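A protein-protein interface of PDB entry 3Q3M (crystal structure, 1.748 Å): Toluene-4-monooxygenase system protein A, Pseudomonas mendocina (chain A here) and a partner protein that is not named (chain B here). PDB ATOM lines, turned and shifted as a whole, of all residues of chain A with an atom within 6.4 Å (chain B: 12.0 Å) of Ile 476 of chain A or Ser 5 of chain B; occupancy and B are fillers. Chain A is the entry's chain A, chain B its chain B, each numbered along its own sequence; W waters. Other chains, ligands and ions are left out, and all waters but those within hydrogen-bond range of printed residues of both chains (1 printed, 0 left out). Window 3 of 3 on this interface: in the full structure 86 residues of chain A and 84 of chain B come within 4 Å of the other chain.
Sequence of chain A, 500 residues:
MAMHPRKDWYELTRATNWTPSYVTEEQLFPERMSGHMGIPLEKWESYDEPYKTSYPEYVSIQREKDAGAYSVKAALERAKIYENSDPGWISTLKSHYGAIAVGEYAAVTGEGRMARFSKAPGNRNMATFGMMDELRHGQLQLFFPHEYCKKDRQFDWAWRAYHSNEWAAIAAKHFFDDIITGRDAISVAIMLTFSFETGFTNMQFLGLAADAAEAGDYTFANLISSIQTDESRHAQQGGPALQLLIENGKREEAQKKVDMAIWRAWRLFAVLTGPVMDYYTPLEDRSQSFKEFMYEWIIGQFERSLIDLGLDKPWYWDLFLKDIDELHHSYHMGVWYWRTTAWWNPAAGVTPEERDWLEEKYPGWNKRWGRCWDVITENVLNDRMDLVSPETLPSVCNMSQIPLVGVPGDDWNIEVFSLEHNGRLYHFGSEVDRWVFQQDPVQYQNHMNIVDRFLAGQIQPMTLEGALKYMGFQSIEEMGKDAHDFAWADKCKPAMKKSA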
ATOM      1  N   GLN A 474      19.442 -26.337  11.356  1.00  0.00           N
ATOM      2  CA  GLN A 474      19.171 -25.300  10.359  1.00  0.00           C
ATOM      3  C   GLN A 474      19.553 -23.907  10.846  1.00  0.00           C
ATOM      4  O   GLN A 474      19.486 -22.947  10.077  1.00  0.00           O
ATOM      5  CB  GLN A 474      17.689 -25.308   9.973  1.00  0.00           C
ATOM      6  CG  GLN A 474      17.267 -26.564   9.192  1.00  0.00           C
ATOM      7  CD  GLN A 474      15.765 -26.663   9.021  1.00  0.00           C
ATOM      8  OE1 GLN A 474      15.048 -25.665   9.126  1.00  0.00           O
ATOM      9  NE2 GLN A 474      15.275 -27.871   8.769  1.00  0.00           N
ATOM     10  N   SER A 475      19.936 -23.781  12.110  1.00  0.00           N
ATOM     11  CA  SER A 475      20.464 -22.496  12.571  1.00  0.00           C
ATOM     12  C   SER A 475      21.328 -22.672  13.795  1.00  0.00           C
ATOM     13  O   SER A 475      21.286 -23.700  14.452  1.00  0.00           O
ATOM     14  CB  SER A 475      19.330 -21.500  12.875  1.00  0.00           C
ATOM     15  OG  SER A 475      18.761 -21.736  14.160  1.00  0.00           O
ATOM     16  N   ILE A 476      22.118 -21.652  14.105  1.00  0.00           N
ATOM     17  CA  ILE A 476      23.029 -21.721  15.235  1.00  0.00           C
ATOM     18  C   ILE A 476      22.271 -21.918  16.553  1.00  0.00           C
ATOM     19  O   ILE A 476      22.734 -22.638  17.432  1.00  0.00           O
ATOM     20  CB  ILE A 476      23.914 -20.451  15.298  1.00  0.00           C
ATOM     21  CG1 ILE A 476      24.894 -20.536  16.463  1.00  0.00           C
ATOM     22  CG2 ILE A 476      23.061 -19.226  15.412  1.00  0.00           C
ATOM     23  CD1 ILE A 476      26.171 -21.277  16.118  1.00  0.00           C
ATOM     24  N   GLU A 477      21.094 -21.296  16.671  1.00  0.00           N
ATOM     25  CA  GLU A 477      20.264 -21.412  17.865  1.00  0.00           C
ATOM     26  C   GLU A 477      19.807 -22.826  18.206  1.00  0.00           C
ATOM     27  O   GLU A 477      19.520 -23.130  19.375  1.00  0.00           O
ATOM     28  CB  GLU A 477      19.022 -20.510  17.744  1.00  0.00           C
ATOM     29  CG  GLU A 477      19.331 -19.016  17.718  1.00  0.00           C
ATOM     30  CD  GLU A 477      19.696 -18.491  16.339  1.00  0.00           C
ATOM     31  OE1 GLU A 477      19.687 -19.266  15.361  1.00  0.00           O
ATOM     32  OE2 GLU A 477      20.010 -17.289  16.234  1.00  0.00           O
ATOM     33  N   GLU A 478      19.720 -23.699  17.197  1.00  0.00           N
ATOM     34  CA  GLU A 478      19.122 -25.017  17.408  1.00  0.00           C
ATOM     35  C   GLU A 478      20.058 -25.993  18.123  1.00  0.00           C
ATOM     36  O   GLU A 478      19.604 -26.937  18.750  1.00  0.00           O
ATOM     37  CB  GLU A 478      18.672 -25.609  16.076  1.00  0.00           C
ATOM     38  CG  GLU A 478      17.672 -24.709  15.369  1.00  0.00           C
ATOM     39  CD  GLU A 478      17.197 -25.294  14.062  1.00  0.00           C
ATOM     40  OE1 GLU A 478      17.719 -26.373  13.676  1.00  0.00           O
ATOM     41  OE2 GLU A 478      16.305 -24.673  13.428  1.00  0.00           O
ATOM     42  N   MET A 479      21.356 -25.759  18.029  1.00  0.00           N
ATOM     43  CA  MET A 479      22.312 -26.680  18.624  1.00  0.00           C
ATOM     44  C   MET A 479      22.388 -26.561  20.136  1.00  0.00           C
ATOM     45  O   MET A 479      22.259 -25.469  20.704  1.00  0.00           O
ATOM     46  CB  MET A 479      23.672 -26.479  17.982  1.00  0.00           C
ATOM     47  CG  MET A 479      23.668 -27.155  16.647  1.00  0.00           C
ATOM     48  SD  MET A 479      25.044 -26.765  15.593  1.00  0.00           S
ATOM     49  CE  MET A 479      24.903 -25.004  15.438  1.00  0.00           C
ATOM     50  N   GLY A 480      22.537 -27.702  20.788  1.00  0.00           N
ATOM     51  CA  GLY A 480      22.548 -27.744  22.241  1.00  0.00           C
ATOM     52  C   GLY A 480      23.673 -26.929  22.853  1.00  0.00           C
ATOM     53  O   GLY A 480      24.800 -26.858  22.325  1.00  0.00           O
ATOM     54  N   LYS A 481      23.367 -26.316  23.983  1.00  0.00           N
ATOM     55  CA  LYS A 481      24.364 -25.597  24.776  1.00  0.00           C
ATOM     56  C   LYS A 481      24.179 -26.006  26.232  1.00  0.00           C
ATOM     57  O   LYS A 481      23.184 -26.631  26.587  1.00  0.00           O
ATOM     58  CB  LYS A 481      24.133 -24.095  24.664  1.00  0.00           C
ATOM     59  CG  LYS A 481      24.336 -23.529  23.259  1.00  0.00           C
ATOM     60  CD  LYS A 481      23.938 -22.041  23.219  1.00  0.00           C
ATOM     61  CE  LYS A 481      24.669 -21.284  22.100  1.00  0.00           C
ATOM     62  NZ  LYS A 481      26.149 -21.172  22.365  1.00  0.00           N
ATOM     63  N   PHE B   3      27.044 -21.520  10.031  1.00  0.00           N
ATOM     64  CA  PHE B   3      25.616 -21.605  10.365  1.00  0.00           C
ATOM     65  C   PHE B   3      24.971 -20.219  10.370  1.00  0.00           C
ATOM     66  O   PHE B   3      25.601 -19.255  10.779  1.00  0.00           O
ATOM     67  CB  PHE B   3      25.421 -22.231  11.744  1.00  0.00           C
ATOM     68  CG  PHE B   3      25.407 -23.728  11.735  1.00  0.00           C
ATOM     69  CD1 PHE B   3      26.519 -24.442  12.125  1.00  0.00           C
ATOM     70  CD2 PHE B   3      24.265 -24.420  11.353  1.00  0.00           C
ATOM     71  CE1 PHE B   3      26.500 -25.826  12.125  1.00  0.00           C
ATOM     72  CE2 PHE B   3      24.239 -25.793  11.349  1.00  0.00           C
ATOM     73  CZ  PHE B   3      25.360 -26.496  11.735  1.00  0.00           C
ATOM     74  N   GLU B   4      23.722 -20.114   9.929  1.00  0.00           N
ATOM     75  CA  GLU B   4      23.010 -18.837  10.004  1.00  0.00           C
ATOM     76  C   GLU B   4      22.277 -18.665  11.330  1.00  0.00           C
ATOM     77  O   GLU B   4      21.961 -19.647  12.010  1.00  0.00           O
ATOM     78  CB  GLU B   4      21.985 -18.717   8.877  1.00  0.00           C
ATOM     79  CG  GLU B   4      22.441 -19.241   7.527  1.00  0.00           C
ATOM     80  CD  GLU B   4      21.270 -19.386   6.570  1.00  0.00           C
ATOM     81  OE1 GLU B   4      20.700 -20.501   6.489  1.00  0.00           O
ATOM     82  OE2 GLU B   4      20.907 -18.373   5.924  1.00  0.00           O
ATOM     83  N   SER B   5      21.972 -17.419  11.686  1.00  0.00           N
ATOM     84  CA  SER B   5      21.155 -17.147  12.869  1.00  0.00           C
ATOM     85  C   SER B   5      19.711 -16.839  12.451  1.00  0.00           C
ATOM     86  O   SER B   5      19.472 -15.913  11.674  1.00  0.00           O
ATOM     87  CB  SER B   5      21.742 -15.972  13.661  1.00  0.00           C
ATOM     88  OG  SER B   5      23.156 -16.072  13.780  1.00  0.00           O
ATOM     89  N   LYS B   6      18.756 -17.603  12.975  1.00  0.00           N
ATOM     90  CA  LYS B   6      17.365 -17.503  12.558  1.00  0.00           C
ATOM     91  C   LYS B   6      16.479 -17.379  13.780  1.00  0.00           C
ATOM     92  O   LYS B   6      16.784 -17.939  14.828  1.00  0.00           O
ATOM     93  CB  LYS B   6      16.945 -18.750  11.781  1.00  0.00           C
ATOM     94  CG  LYS B   6      17.735 -18.976  10.505  1.00  0.00           C
ATOM     95  CD  LYS B   6      17.180 -20.166   9.737  1.00  0.00           C
ATOM     96  CE  LYS B   6      18.012 -20.392   8.470  1.00  0.00           C
ATOM     97  NZ  LYS B   6      17.782 -21.742   7.871  1.00  0.00           N
ATOM     98  N   LYS B   7      15.396 -16.625  13.638  1.00  0.00           N
ATOM     99  CA  LYS B   7      14.448 -16.414  14.719  1.00  0.00           C
ATOM    100  C   LYS B   7      13.483 -17.591  14.878  1.00  0.00           C
ATOM    101  O   LYS B   7      13.322 -18.417  13.979  1.00  0.00           O
ATOM    102  CB  LYS B   7      13.652 -15.123  14.462  1.00  0.00           C
ATOM    103  CG  LYS B   7      14.534 -13.880  14.249  1.00  0.00           C
ATOM    104  CD  LYS B   7      15.755 -13.872  15.186  1.00  0.00           C
ATOM    105  CE  LYS B   7      16.966 -13.091  14.592  1.00  0.00           C
ATOM    106  NZ  LYS B   7      17.806 -13.837  13.584  1.00  0.00           N
ATOM    107  N   PRO B   8      12.832 -17.677  16.044  1.00  0.00           N
ATOM    108  CA  PRO B   8      11.777 -18.690  16.209  1.00  0.00           C
ATOM    109  C   PRO B   8      10.679 -18.517  15.170  1.00  0.00           C
ATOM    110  O   PRO B   8      10.395 -17.388  14.759  1.00  0.00           O
ATOM    111  CB  PRO B   8      11.215 -18.383  17.596  1.00  0.00           C
ATOM    112  CG  PRO B   8      12.414 -17.801  18.338  1.00  0.00           C
ATOM    113  CD  PRO B   8      13.067 -16.918  17.282  1.00  0.00           C
ATOM    114  N   MET B   9      10.073 -19.635  14.767  1.00  0.00           N
ATOM    115  CA  MET B   9       8.989 -19.660  13.788  1.00  0.00           C
ATOM    116  C   MET B   9       7.635 -19.729  14.500  1.00  0.00           C
ATOM    117  O   MET B   9       7.548 -20.194  15.622  1.00  0.00           O
ATOM    118  CB  MET B   9       9.169 -20.859  12.844  1.00  0.00           C
ATOM    119  CG  MET B   9      10.447 -20.733  11.983  1.00  0.00           C
ATOM    120  SD  MET B   9      11.022 -22.261  11.230  1.00  0.00           S
ATOM    121  CE  MET B   9      11.537 -23.217  12.663  1.00  0.00           C
HETATM  122  O   HOH W   1      13.767 -23.294   9.125  1.00  0.00           O
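The backbone carbonyl oxygen (O) of Glu 4 of chain B is in hydrogen-bond range of the backbone NH (N) of Ile 476 of chain A, at 2.9 Å.
O of Gln 474 of chain A lies within hydrogen-bond range of NZ of Lys 6 of chain B, at 3.0 Å.
The side-chain carboxylate of Glu 477 of chain A lies within hydrogen-bond range of the backbone NH of Lys 6 of chain B, at 3.1 Å.
The side-chain carboxylate of Glu 477 of chain A lies within hydrogen-bond range of the side-chain hydroxyl of Ser 475 of chain A (2.9 Å).
The side-chain carboxylate of Glu 478 of chain A sits at hydrogen-bond distance from the backbone NH of Gln 474 of chain A, 2.9 Å away.
O of Ser 5 of chain B is in hydrogen-bond range of NZ of Lys 7 of chain B, at 3.3 Å.
The side-chain carboxylate (OE1) of Glu 4 of chain B is in salt-bridge range of the side-chain amino group (NZ) of Lys 6 of chain B (3.5 Å).
Ser 475 of chain A touches Glu 4 of chain B.
Lys 6 of chain B touches Ser 475 of chain A.
Ile 476 of chain A touches Ser 5 of chain B.
OE2 of Glu 477 of chain A touches CB of Ser 5 of chain B, 3.4 Å away.
Phe 3 of chain B touches Met 479 of chain A.
Printed residues of chain B within 4 Å of Ile 476 of chain A: Glu 4 (2.9 Å) and Ser 5 (3.6 Å).
Of the printed residues of chain A, Ser 5 of chain B touches Ile 476 (3.6 Å) and Glu 477 (3.4 Å).
Ser 475 of chain A touches just these residues of chain B: Glu 4 (3.3 Å) and Lys 6 (3.8 Å).
No residue of chain B comes within 4 Å of Glu 478 of chain A.
Of chain B, only Phe 3 comes within 4 Å of Met 479 of chain A.
No residue of chain B comes within 4 Å of Gly 480 of chain A.
Of the printed residues of chain A, Glu 4 of chain B touches Ser 475 (3.3 Å) and Ile 476 (2.9 Å).
Printed residues of chain B within 4 Å of Glu 477 of chain A: Ser 5 and Lys 6.
Pro 8 of chain B touches none of the printed residues of chain A.
Met 9 of chain B touches none of the printed residues of chain A.
The nearest printed residue of chain A that does not touch Lys 6 of chain B is Ile 476 of chain A (5.2 Å).
Hydrophobic or aromatic side chains of chain A that line the printed part of chain B: Ile 476 and Met 479.
Among the printed residues, 8 pairs touch across the chains.
Water W1 lies within hydrogen-bond range of OE1 of Gln 474 of chain A and SD of Met 9 of chain B.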
